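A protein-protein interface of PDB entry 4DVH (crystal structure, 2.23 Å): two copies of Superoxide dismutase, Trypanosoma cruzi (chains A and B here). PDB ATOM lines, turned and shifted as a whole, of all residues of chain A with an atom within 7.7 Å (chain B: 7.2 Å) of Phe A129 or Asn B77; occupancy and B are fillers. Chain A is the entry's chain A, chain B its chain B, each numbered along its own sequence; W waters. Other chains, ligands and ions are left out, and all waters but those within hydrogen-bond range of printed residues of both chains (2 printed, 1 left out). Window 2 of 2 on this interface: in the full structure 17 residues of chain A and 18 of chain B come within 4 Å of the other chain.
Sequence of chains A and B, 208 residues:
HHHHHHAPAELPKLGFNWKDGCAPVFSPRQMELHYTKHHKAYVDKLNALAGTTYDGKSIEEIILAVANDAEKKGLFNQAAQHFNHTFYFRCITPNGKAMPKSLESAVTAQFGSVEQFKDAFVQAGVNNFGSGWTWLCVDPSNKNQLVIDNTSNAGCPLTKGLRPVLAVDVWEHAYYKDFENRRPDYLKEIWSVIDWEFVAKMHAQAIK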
ATOM      1  N   ALA A 124      15.191 -20.973  29.432  1.00  0.00           N
ATOM      2  CA  ALA A 124      16.471 -21.356  30.017  1.00  0.00           C
ATOM      3  C   ALA A 124      17.491 -21.731  28.927  1.00  0.00           C
ATOM      4  O   ALA A 124      18.633 -21.288  28.984  1.00  0.00           O
ATOM      5  CB  ALA A 124      16.272 -22.503  30.998  1.00  0.00           C
ATOM      6  N   GLY A 125      17.057 -22.505  27.933  1.00  0.00           N
ATOM      7  CA  GLY A 125      17.902 -22.936  26.816  1.00  0.00           C
ATOM      8  C   GLY A 125      18.372 -21.789  25.949  1.00  0.00           C
ATOM      9  O   GLY A 125      19.555 -21.685  25.644  1.00  0.00           O
ATOM     10  N   VAL A 126      17.451 -20.898  25.591  1.00  0.00           N
ATOM     11  CA  VAL A 126      17.691 -19.690  24.783  1.00  0.00           C
ATOM     12  C   VAL A 126      18.725 -18.781  25.459  1.00  0.00           C
ATOM     13  O   VAL A 126      19.588 -18.230  24.783  1.00  0.00           O
ATOM     14  CB  VAL A 126      16.365 -18.932  24.466  1.00  0.00           C
ATOM     15  CG1 VAL A 126      16.642 -17.578  23.817  1.00  0.00           C
ATOM     16  CG2 VAL A 126      15.466 -19.768  23.559  1.00  0.00           C
ATOM     17  N   ASN A 127      18.637 -18.647  26.792  1.00  0.00           N
ATOM     18  CA  ASN A 127      19.526 -17.787  27.565  1.00  0.00           C
ATOM     19  C   ASN A 127      20.773 -18.464  28.128  1.00  0.00           C
ATOM     20  O   ASN A 127      21.540 -17.825  28.861  1.00  0.00           O
ATOM     21  CB  ASN A 127      18.739 -17.057  28.644  1.00  0.00           C
ATOM     22  CG  ASN A 127      17.655 -16.204  28.043  1.00  0.00           C
ATOM     23  OD1 ASN A 127      17.903 -15.288  27.252  1.00  0.00           O
ATOM     24  ND2 ASN A 127      16.429 -16.556  28.329  1.00  0.00           N
ATOM     25  N   ASN A 128      20.996 -19.732  27.770  1.00  0.00           N
ATOM     26  CA  ASN A 128      22.176 -20.456  28.221  1.00  0.00           C
ATOM     27  C   ASN A 128      23.315 -20.024  27.252  1.00  0.00           C
ATOM     28  O   ASN A 128      23.407 -20.523  26.122  1.00  0.00           O
ATOM     29  CB  ASN A 128      21.926 -21.998  28.213  1.00  0.00           C
ATOM     30  CG  ASN A 128      22.928 -22.774  29.037  1.00  0.00           C
ATOM     31  OD1 ASN A 128      23.930 -22.237  29.491  1.00  0.00           O
ATOM     32  ND2 ASN A 128      22.677 -24.056  29.277  1.00  0.00           N
ATOM     33  N   PHE A 129      24.118 -19.029  27.687  1.00  0.00           N
ATOM     34  CA  PHE A 129      25.182 -18.433  26.902  1.00  0.00           C
ATOM     35  C   PHE A 129      26.322 -19.382  26.523  1.00  0.00           C
ATOM     36  O   PHE A 129      26.967 -19.990  27.395  1.00  0.00           O
ATOM     37  CB  PHE A 129      25.706 -17.146  27.553  1.00  0.00           C
ATOM     38  CG  PHE A 129      26.549 -16.330  26.600  1.00  0.00           C
ATOM     39  CD1 PHE A 129      25.958 -15.598  25.573  1.00  0.00           C
ATOM     40  CD2 PHE A 129      27.934 -16.323  26.701  1.00  0.00           C
ATOM     41  CE1 PHE A 129      26.743 -14.869  24.673  1.00  0.00           C
ATOM     42  CE2 PHE A 129      28.713 -15.575  25.807  1.00  0.00           C
ATOM     43  CZ  PHE A 129      28.114 -14.881  24.785  1.00  0.00           C
ATOM     44  N   GLY A 130      26.586 -19.441  25.218  1.00  0.00           N
ATOM     45  CA  GLY A 130      27.626 -20.286  24.645  1.00  0.00           C
ATOM     46  C   GLY A 130      27.208 -21.737  24.565  1.00  0.00           C
ATOM     47  O   GLY A 130      26.030 -22.034  24.340  1.00  0.00           O
ATOM     48  N   SER A 131      28.187 -22.648  24.745  1.00  0.00           N
ATOM     49  CA  SER A 131      27.963 -24.092  24.722  1.00  0.00           C
ATOM     50  C   SER A 131      27.423 -24.528  26.077  1.00  0.00           C
ATOM     51  O   SER A 131      27.940 -24.097  27.104  1.00  0.00           O
ATOM     52  CB  SER A 131      29.263 -24.821  24.415  1.00  0.00           C
ATOM     53  OG  SER A 131      29.741 -24.472  23.125  1.00  0.00           O
ATOM     54  N   GLY A 132      26.388 -25.374  26.069  1.00  0.00           N
ATOM     55  CA  GLY A 132      25.802 -25.877  27.302  1.00  0.00           C
ATOM     56  C   GLY A 132      24.708 -26.912  27.168  1.00  0.00           C
ATOM     57  O   GLY A 132      24.482 -27.516  26.106  1.00  0.00           O
ATOM     58  N   ASN A 150      20.557 -25.074  34.098  1.00  0.00           N
ATOM     59  CA  ASN A 150      21.455 -24.763  32.988  1.00  0.00           C
ATOM     60  C   ASN A 150      22.883 -25.065  33.400  1.00  0.00           C
ATOM     61  O   ASN A 150      23.299 -24.691  34.506  1.00  0.00           O
ATOM     62  CB  ASN A 150      21.373 -23.283  32.621  1.00  0.00           C
ATOM     63  CG  ASN A 150      20.326 -22.961  31.612  1.00  0.00           C
ATOM     64  OD1 ASN A 150      19.777 -23.836  30.937  1.00  0.00           O
ATOM     65  ND2 ASN A 150      20.067 -21.681  31.443  1.00  0.00           N
ATOM     66  N   THR A 151      23.618 -25.769  32.527  1.00  0.00           N
ATOM     67  CA  THR A 151      25.040 -26.037  32.732  1.00  0.00           C
ATOM     68  C   THR A 151      25.815 -25.496  31.521  1.00  0.00           C
ATOM     69  O   THR A 151      25.261 -25.374  30.414  1.00  0.00           O
ATOM     70  CB  THR A 151      25.348 -27.506  33.069  1.00  0.00           C
ATOM     71  OG1 THR A 151      24.959 -28.383  32.007  1.00  0.00           O
ATOM     72  CG2 THR A 151      24.753 -27.954  34.420  1.00  0.00           C
ATOM     73  N   SER A 152      27.069 -25.099  31.759  1.00  0.00           N
ATOM     74  CA  SER A 152      27.937 -24.547  30.719  1.00  0.00           C
ATOM     75  C   SER A 152      28.945 -25.620  30.306  1.00  0.00           C
ATOM     76  O   SER A 152      29.405 -26.399  31.145  1.00  0.00           O
ATOM     77  CB  SER A 152      28.650 -23.282  31.216  1.00  0.00           C
ATOM     78  OG  SER A 152      29.719 -22.905  30.357  1.00  0.00           O
ATOM     79  N   ASN A 153      29.261 -25.666  29.017  1.00  0.00           N
ATOM     80  CA  ASN A 153      30.212 -26.618  28.434  1.00  0.00           C
ATOM     81  C   ASN A 153      29.901 -28.087  28.748  1.00  0.00           C
ATOM     82  O   ASN A 153      28.884 -28.598  28.258  1.00  0.00           O
ATOM     83  CB  ASN A 153      31.673 -26.196  28.749  1.00  0.00           C
ATOM     84  CG  ASN A 153      32.042 -24.917  28.041  1.00  0.00           C
ATOM     85  OD1 ASN A 153      31.404 -24.525  27.056  1.00  0.00           O
ATOM     86  ND2 ASN A 153      33.080 -24.255  28.502  1.00  0.00           N
ATOM     87  N   VAL A 170      22.527 -27.749  24.076  1.00  0.00           N
ATOM     88  CA  VAL A 170      22.476 -26.412  23.467  1.00  0.00           C
ATOM     89  C   VAL A 170      23.830 -25.973  22.881  1.00  0.00           C
ATOM     90  O   VAL A 170      24.001 -24.809  22.507  1.00  0.00           O
ATOM     91  CB  VAL A 170      21.678 -25.307  24.231  1.00  0.00           C
ATOM     92  CG1 VAL A 170      20.227 -25.710  24.413  1.00  0.00           C
ATOM     93  CG2 VAL A 170      22.316 -24.946  25.574  1.00  0.00           C
ATOM     94  N   ARG A 183      18.539 -21.371  17.476  1.00  0.00           N
ATOM     95  CA  ARG A 183      18.395 -22.105  18.736  1.00  0.00           C
ATOM     96  C   ARG A 183      16.946 -22.055  19.291  1.00  0.00           C
ATOM     97  O   ARG A 183      16.476 -23.119  19.703  1.00  0.00           O
ATOM     98  CB  ARG A 183      19.392 -21.640  19.803  1.00  0.00           C
ATOM     99  CG  ARG A 183      19.434 -22.612  20.983  1.00  0.00           C
ATOM    100  CD  ARG A 183      20.081 -21.990  22.180  1.00  0.00           C
ATOM    101  NE  ARG A 183      21.513 -22.006  21.994  1.00  0.00           N
ATOM    102  CZ  ARG A 183      22.389 -21.738  22.937  1.00  0.00           C
ATOM    103  NH1 ARG A 183      21.980 -21.397  24.153  1.00  0.00           N
ATOM    104  NH2 ARG A 183      23.690 -21.829  22.682  1.00  0.00           N
ATOM    105  N   TYR B  42      24.181  -9.850  18.267  1.00  0.00           N
ATOM    106  CA  TYR B  42      25.030  -9.293  19.334  1.00  0.00           C
ATOM    107  C   TYR B  42      24.874  -7.780  19.351  1.00  0.00           C
ATOM    108  O   TYR B  42      24.725  -7.189  20.422  1.00  0.00           O
ATOM    109  CB  TYR B  42      26.524  -9.681  19.143  1.00  0.00           C
ATOM    110  CG  TYR B  42      26.825 -11.131  19.451  1.00  0.00           C
ATOM    111  CD1 TYR B  42      26.486 -11.691  20.689  1.00  0.00           C
ATOM    112  CD2 TYR B  42      27.425 -11.953  18.505  1.00  0.00           C
ATOM    113  CE1 TYR B  42      26.750 -13.034  20.971  1.00  0.00           C
ATOM    114  CE2 TYR B  42      27.673 -13.299  18.766  1.00  0.00           C
ATOM    115  CZ  TYR B  42      27.360 -13.829  20.009  1.00  0.00           C
ATOM    116  OH  TYR B  42      27.651 -15.147  20.277  1.00  0.00           O
ATOM    117  N   LEU B  46      23.184  -5.776  22.416  1.00  0.00           N
ATOM    118  CA  LEU B  46      24.063  -4.787  23.031  1.00  0.00           C
ATOM    119  C   LEU B  46      23.329  -3.447  23.103  1.00  0.00           C
ATOM    120  O   LEU B  46      23.270  -2.858  24.170  1.00  0.00           O
ATOM    121  CB  LEU B  46      25.382  -4.673  22.217  1.00  0.00           C
ATOM    122  CG  LEU B  46      26.295  -3.477  22.452  1.00  0.00           C
ATOM    123  CD1 LEU B  46      26.728  -3.364  23.908  1.00  0.00           C
ATOM    124  CD2 LEU B  46      27.490  -3.556  21.549  1.00  0.00           C
ATOM    125  N   LEU B  49      20.608  -3.630  25.834  1.00  0.00           N
ATOM    126  CA  LEU B  49      21.112  -3.626  27.217  1.00  0.00           C
ATOM    127  C   LEU B  49      21.876  -2.351  27.611  1.00  0.00           C
ATOM    128  O   LEU B  49      21.914  -1.995  28.791  1.00  0.00           O
ATOM    129  CB  LEU B  49      21.990  -4.867  27.483  1.00  0.00           C
ATOM    130  CG  LEU B  49      21.310  -6.219  27.329  1.00  0.00           C
ATOM    131  CD1 LEU B  49      22.330  -7.332  27.399  1.00  0.00           C
ATOM    132  CD2 LEU B  49      20.229  -6.405  28.391  1.00  0.00           C
ATOM    133  N   VAL B  66      32.201  -2.758  32.582  1.00  0.00           N
ATOM    134  CA  VAL B  66      31.256  -3.803  32.917  1.00  0.00           C
ATOM    135  C   VAL B  66      31.905  -5.174  33.194  1.00  0.00           C
ATOM    136  O   VAL B  66      31.265  -6.029  33.804  1.00  0.00           O
ATOM    137  CB  VAL B  66      30.192  -3.750  31.798  1.00  0.00           C
ATOM    138  CG1 VAL B  66      29.475  -5.050  31.591  1.00  0.00           C
ATOM    139  CG2 VAL B  66      29.213  -2.606  32.046  1.00  0.00           C
ATOM    140  N   LYS B  72      26.099  -7.112  35.500  1.00  0.00           N
ATOM    141  CA  LYS B  72      26.093  -6.676  34.099  1.00  0.00           C
ATOM    142  C   LYS B  72      26.797  -7.667  33.167  1.00  0.00           C
ATOM    143  O   LYS B  72      27.339  -7.274  32.135  1.00  0.00           O
ATOM    144  CB  LYS B  72      26.658  -5.245  33.967  1.00  0.00           C
ATOM    145  CG  LYS B  72      25.815  -4.183  34.661  1.00  0.00           C
ATOM    146  CD  LYS B  72      26.492  -2.823  34.634  1.00  0.00           C
ATOM    147  CE  LYS B  72      25.705  -1.738  35.336  1.00  0.00           C
ATOM    148  NZ  LYS B  72      25.810  -1.833  36.816  1.00  0.00           N
ATOM    149  N   LYS B  73      26.735  -8.967  33.510  1.00  0.00           N
ATOM    150  CA  LYS B  73      27.303 -10.051  32.714  1.00  0.00           C
ATOM    151  C   LYS B  73      26.680 -10.112  31.307  1.00  0.00           C
ATOM    152  O   LYS B  73      27.416 -10.328  30.337  1.00  0.00           O
ATOM    153  CB  LYS B  73      27.188 -11.400  33.435  1.00  0.00           C
ATOM    154  CG  LYS B  73      28.264 -11.624  34.473  1.00  0.00           C
ATOM    155  CD  LYS B  73      28.057 -12.953  35.164  1.00  0.00           C
ATOM    156  CE  LYS B  73      29.091 -13.178  36.229  1.00  0.00           C
ATOM    157  NZ  LYS B  73      28.911 -14.494  36.887  1.00  0.00           N
ATOM    158  N   GLY B  74      25.360  -9.885  31.210  1.00  0.00           N
ATOM    159  CA  GLY B  74      24.623  -9.855  29.942  1.00  0.00           C
ATOM    160  C   GLY B  74      25.198  -8.824  28.998  1.00  0.00           C
ATOM    161  O   GLY B  74      25.527  -9.126  27.848  1.00  0.00           O
ATOM    162  N   LEU B  75      25.357  -7.594  29.502  1.00  0.00           N
ATOM    163  CA  LEU B  75      25.945  -6.480  28.766  1.00  0.00           C
ATOM    164  C   LEU B  75      27.409  -6.783  28.391  1.00  0.00           C
ATOM    165  O   LEU B  75      27.778  -6.555  27.240  1.00  0.00           O
ATOM    166  CB  LEU B  75      25.839  -5.180  29.581  1.00  0.00           C
ATOM    167  CG  LEU B  75      26.420  -3.911  28.948  1.00  0.00           C
ATOM    168  CD1 LEU B  75      25.828  -3.627  27.550  1.00  0.00           C
ATOM    169  CD2 LEU B  75      26.201  -2.746  29.851  1.00  0.00           C
ATOM    170  N   PHE B  76      28.205  -7.347  29.327  1.00  0.00           N
ATOM    171  CA  PHE B  76      29.603  -7.719  29.051  1.00  0.00           C
ATOM    172  C   PHE B  76      29.647  -8.671  27.851  1.00  0.00           C
ATOM    173  O   PHE B  76      30.414  -8.431  26.912  1.00  0.00           O
ATOM    174  CB  PHE B  76      30.316  -8.362  30.282  1.00  0.00           C
ATOM    175  CG  PHE B  76      31.698  -8.863  29.927  1.00  0.00           C
ATOM    176  CD1 PHE B  76      32.798  -8.009  29.966  1.00  0.00           C
ATOM    177  CD2 PHE B  76      31.894 -10.174  29.468  1.00  0.00           C
ATOM    178  CE1 PHE B  76      34.070  -8.458  29.562  1.00  0.00           C
ATOM    179  CE2 PHE B  76      33.155 -10.606  29.036  1.00  0.00           C
ATOM    180  CZ  PHE B  76      34.234  -9.745  29.085  1.00  0.00           C
ATOM    181  N   ASN B  77      28.838  -9.759  27.903  1.00  0.00           N
ATOM    182  CA  ASN B  77      28.769 -10.767  26.839  1.00  0.00           C
ATOM    183  C   ASN B  77      28.486 -10.177  25.471  1.00  0.00           C
ATOM    184  O   ASN B  77      29.174 -10.513  24.521  1.00  0.00           O
ATOM    185  CB  ASN B  77      27.745 -11.864  27.181  1.00  0.00           C
ATOM    186  CG  ASN B  77      28.175 -12.766  28.299  1.00  0.00           C
ATOM    187  OD1 ASN B  77      29.359 -12.874  28.630  1.00  0.00           O
ATOM    188  ND2 ASN B  77      27.219 -13.462  28.897  1.00  0.00           N
ATOM    189  N   GLN B  78      27.475  -9.310  25.366  1.00  0.00           N
ATOM    190  CA  GLN B  78      27.102  -8.707  24.080  1.00  0.00           C
ATOM    191  C   GLN B  78      28.160  -7.709  23.600  1.00  0.00           C
ATOM    192  O   GLN B  78      28.516  -7.735  22.432  1.00  0.00           O
ATOM    193  CB  GLN B  78      25.685  -8.079  24.132  1.00  0.00           C
ATOM    194  CG  GLN B  78      24.574  -9.014  24.658  1.00  0.00           C
ATOM    195  CD  GLN B  78      24.424 -10.315  23.884  1.00  0.00           C
ATOM    196  OE1 GLN B  78      24.267 -10.330  22.673  1.00  0.00           O
ATOM    197  NE2 GLN B  78      24.448 -11.439  24.567  1.00  0.00           N
ATOM    198  N   ALA B  79      28.677  -6.865  24.512  1.00  0.00           N
ATOM    199  CA  ALA B  79      29.685  -5.869  24.148  1.00  0.00           C
ATOM    200  C   ALA B  79      30.993  -6.538  23.747  1.00  0.00           C
ATOM    201  O   ALA B  79      31.573  -6.153  22.723  1.00  0.00           O
ATOM    202  CB  ALA B  79      29.910  -4.868  25.271  1.00  0.00           C
ATOM    203  N   ALA B  80      31.441  -7.572  24.506  1.00  0.00           N
ATOM    204  CA  ALA B  80      32.692  -8.254  24.152  1.00  0.00           C
ATOM    205  C   ALA B  80      32.559  -9.002  22.850  1.00  0.00           C
ATOM    206  O   ALA B  80      33.494  -8.958  22.046  1.00  0.00           O
ATOM    207  CB  ALA B  80      33.142  -9.172  25.257  1.00  0.00           C
ATOM    208  N   GLN B  81      31.387  -9.640  22.598  1.00  0.00           N
ATOM    209  CA  GLN B  81      31.153 -10.365  21.350  1.00  0.00           C
ATOM    210  C   GLN B  81      31.100  -9.443  20.147  1.00  0.00           C
ATOM    211  O   GLN B  81      31.546  -9.838  19.076  1.00  0.00           O
ATOM    212  CB  GLN B  81      29.903 -11.279  21.425  1.00  0.00           C
ATOM    213  CG  GLN B  81      30.090 -12.564  22.277  1.00  0.00           C
ATOM    214  CD  GLN B  81      31.081 -13.522  21.678  1.00  0.00           C
ATOM    215  OE1 GLN B  81      32.284 -13.374  21.840  1.00  0.00           O
ATOM    216  NE2 GLN B  81      30.589 -14.539  20.977  1.00  0.00           N
ATOM    217  N   HIS B  82      30.567  -8.223  20.307  1.00  0.00           N
ATOM    218  CA  HIS B  82      30.515  -7.276  19.193  1.00  0.00           C
ATOM    219  C   HIS B  82      31.947  -6.878  18.840  1.00  0.00           C
ATOM    220  O   HIS B  82      32.302  -6.895  17.660  1.00  0.00           O
ATOM    221  CB  HIS B  82      29.610  -6.049  19.500  1.00  0.00           C
ATOM    222  CG  HIS B  82      29.729  -4.916  18.502  1.00  0.00           C
ATOM    223  ND1 HIS B  82      29.702  -5.144  17.133  1.00  0.00           N
ATOM    224  CD2 HIS B  82      29.793  -3.579  18.716  1.00  0.00           C
ATOM    225  CE1 HIS B  82      29.759  -3.952  16.565  1.00  0.00           C
ATOM    226  NE2 HIS B  82      29.809  -2.979  17.475  1.00  0.00           N
ATOM    227  N   PHE B  83      32.776  -6.577  19.858  1.00  0.00           N
ATOM    228  CA  PHE B  83      34.215  -6.250  19.666  1.00  0.00           C
ATOM    229  C   PHE B  83      34.959  -7.440  18.985  1.00  0.00           C
ATOM    230  O   PHE B  83      35.570  -7.298  17.915  1.00  0.00           O
ATOM    231  CB  PHE B  83      34.892  -5.873  21.004  1.00  0.00           C
ATOM    232  CG  PHE B  83      36.400  -5.705  20.903  1.00  0.00           C
ATOM    233  CD1 PHE B  83      36.958  -4.484  20.545  1.00  0.00           C
ATOM    234  CD2 PHE B  83      37.256  -6.787  21.111  1.00  0.00           C
ATOM    235  CE1 PHE B  83      38.341  -4.351  20.372  1.00  0.00           C
ATOM    236  CE2 PHE B  83      38.641  -6.653  20.942  1.00  0.00           C
ATOM    237  CZ  PHE B  83      39.175  -5.434  20.578  1.00  0.00           C
ATOM    238  N   ASN B  84      34.813  -8.616  19.565  1.00  0.00           N
ATOM    239  CA  ASN B  84      35.444  -9.844  19.056  1.00  0.00           C
ATOM    240  C   ASN B  84      35.106 -10.141  17.618  1.00  0.00           C
ATOM    241  O   ASN B  84      36.014 -10.467  16.848  1.00  0.00           O
ATOM    242  CB  ASN B  84      35.095 -11.028  19.951  1.00  0.00           C
ATOM    243  CG  ASN B  84      35.652 -10.952  21.357  1.00  0.00           C
ATOM    244  OD1 ASN B  84      36.452 -10.095  21.686  1.00  0.00           O
ATOM    245  ND2 ASN B  84      35.167 -11.799  22.247  1.00  0.00           N
ATOM    246  N   SER B 131      32.867 -23.035  23.346  1.00  0.00           N
ATOM    247  CA  SER B 131      32.829 -21.811  22.563  1.00  0.00           C
ATOM    248  C   SER B 131      33.960 -20.912  23.036  1.00  0.00           C
ATOM    249  O   SER B 131      34.184 -20.790  24.252  1.00  0.00           O
ATOM    250  CB  SER B 131      31.487 -21.122  22.766  1.00  0.00           C
ATOM    251  OG  SER B 131      30.440 -21.933  22.261  1.00  0.00           O
ATOM    252  N   SER B 152      37.378 -18.034  26.602  1.00  0.00           N
ATOM    253  CA  SER B 152      36.169 -18.846  26.600  1.00  0.00           C
ATOM    254  C   SER B 152      34.958 -17.923  26.424  1.00  0.00           C
ATOM    255  O   SER B 152      34.940 -16.809  26.955  1.00  0.00           O
ATOM    256  CB  SER B 152      36.066 -19.643  27.908  1.00  0.00           C
ATOM    257  OG  SER B 152      34.781 -20.223  28.070  1.00  0.00           O
ATOM    258  N   ASN B 153      33.963 -18.392  25.659  1.00  0.00           N
ATOM    259  CA  ASN B 153      32.716 -17.666  25.394  1.00  0.00           C
ATOM    260  C   ASN B 153      32.928 -16.263  24.818  1.00  0.00           C
ATOM    261  O   ASN B 153      33.405 -16.151  23.673  1.00  0.00           O
ATOM    262  CB  ASN B 153      31.776 -17.720  26.622  1.00  0.00           C
ATOM    263  CG  ASN B 153      31.274 -19.117  26.873  1.00  0.00           C
ATOM    264  OD1 ASN B 153      31.305 -19.969  25.996  1.00  0.00           O
ATOM    265  ND2 ASN B 153      30.789 -19.382  28.064  1.00  0.00           N
ATOM    266  N   ALA B 154      32.602 -15.203  25.608  1.00  0.00           N
ATOM    267  CA  ALA B 154      32.765 -13.803  25.209  1.00  0.00           C
ATOM    268  C   ALA B 154      34.098 -13.226  25.681  1.00  0.00           C
ATOM    269  O   ALA B 154      34.390 -12.076  25.363  1.00  0.00           O
ATOM    270  CB  ALA B 154      31.603 -12.955  25.732  1.00  0.00           C
ATOM    271  N   GLY B 155      34.905 -14.030  26.394  1.00  0.00           N
ATOM    272  CA  GLY B 155      36.223 -13.642  26.891  1.00  0.00           C
ATOM    273  C   GLY B 155      36.991 -12.754  25.925  1.00  0.00           C
ATOM    274  O   GLY B 155      37.095 -13.058  24.729  1.00  0.00           O
ATOM    275  N   TRP B 171      33.898 -20.557  18.182  1.00  0.00           N
ATOM    276  CA  TRP B 171      32.509 -20.889  18.504  1.00  0.00           C
ATOM    277  C   TRP B 171      32.142 -21.737  17.287  1.00  0.00           C
ATOM    278  O   TRP B 171      32.609 -21.441  16.186  1.00  0.00           O
ATOM    279  CB  TRP B 171      31.629 -19.627  18.522  1.00  0.00           C
ATOM    280  CG  TRP B 171      31.598 -18.873  19.829  1.00  0.00           C
ATOM    281  CD1 TRP B 171      32.624 -18.165  20.396  1.00  0.00           C
ATOM    282  CD2 TRP B 171      30.435 -18.593  20.616  1.00  0.00           C
ATOM    283  NE1 TRP B 171      32.182 -17.515  21.534  1.00  0.00           N
ATOM    284  CE2 TRP B 171      30.839 -17.757  21.688  1.00  0.00           C
ATOM    285  CE3 TRP B 171      29.095 -19.004  20.547  1.00  0.00           C
ATOM    286  CZ2 TRP B 171      29.946 -17.328  22.687  1.00  0.00           C
ATOM    287  CZ3 TRP B 171      28.207 -18.565  21.528  1.00  0.00           C
ATOM    288  CH2 TRP B 171      28.636 -17.747  22.584  1.00  0.00           C
HETATM  289  O   HOH W   1      34.369 -22.336  26.438  1.00  0.00           O
HETATM  290  O   HOH W   2      28.808 -21.846  28.089  1.00  0.00           O
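Phe A129 touches just these residues of chain B: Asn B77, Gln B81, Asn B153, Ala B154 and Trp B171.
Of chain A, only Phe A129 comes within 4 Å of Asn B77.
Of the printed residues of chain A, Asn B153 touches Phe A129 (3.8 Å) and Gly A130 (3.9 Å).
Printed residues of chain A within 4 Å of Ala B154: Phe A129.
Of the printed residues of chain A, Ser B131 touches Gly A130 and Ser A131.
Printed residues of chain B within 4 Å of Gly A130: Ser B131, Asn B153 and Trp B171.
Of the printed residues of chain A, Trp B171 touches Phe A129 (3.7 Å) and Gly A130 (3.4 Å).
The nearest residue of chain A that does not touch Asn B77 is Gly A130 (7.0 Å).
The nearest printed residue of chain A that does not touch Asn B153 is Ser A131 (4.3 Å).
Printed residues of chain B that touch a printed residue of chain A: Asn B77, Gln B81, Ser B131, Asn B153, Ala B154 and Trp B171.
Hydrophobic or aromatic side chains of chain B within 4 Å of the printed part of chain A: Ala B154 and Trp B171.
Of the 15 printed residues of chain A, 3 touch a printed residue of chain B.
Hydrophobic or aromatic side chains of chain A that line the printed part of chain B: Phe A129.
Along chain A the printed residues that touch a printed residue of chain B span positions 129 to 131.
Among the printed residues, no Asp or Glu carboxylate lies within 4 Å of a Lys or Arg side-chain nitrogen of the other chain.
Among the printed residues, merely in contact across the chains: Gly A130 with Trp B171, Phe A129 with Trp B171, Phe A129 with Asn B77, Phe A129 with Asn B153, Phe A129 with Ala B154, Gly A130 with Asn B153, Phe A129 with Gln B81 and Gly A130 with Ser B131.
Water W2 lies within hydrogen-bond range of O of Ser A131 (2.6 Å), OG of Ser A152 (2.7 Å), O of Phe A129 (2.7 Å) and ND2 of Asn B153 (3.2 Å).
Water W1 lies within hydrogen-bond range of O of Ser B131 (2.7 Å), OG of Ser B152 (2.7 Å) and ND2 of Asn A153 (3.1 Å).
Ser A131 touches its own counterpart, Ser B131.
Of the 9 pairs that touch across the chains among the printed residues, 1 has its exchanged pair printed and touching as well.
OG of Ser B131 sits at hydrogen-bond distance from OG of Ser A131, 2.8 Å away.
OE1 of Gln B81 is in hydrogen-bond range of ND2 of Asn B84 (3.3 Å).
ND2 of Asn B77 lies close to O of Lys B73 (3.5 Å).
O of Gly A130 sits at hydrogen-bond distance from NH2 of Arg A183 (2.9 Å).
The backbone carbonyl oxygen of Asn B153 is in hydrogen-bond range of the indole nitrogen of Trp B171 (2.8 Å).
The backbone carbonyl oxygen of Ser A131 lies within hydrogen-bond range of the backbone NH of Asn A153 (2.8 Å).
NE1 of Trp B171 lies close to NE2 of Gln B81 (3.4 Å).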
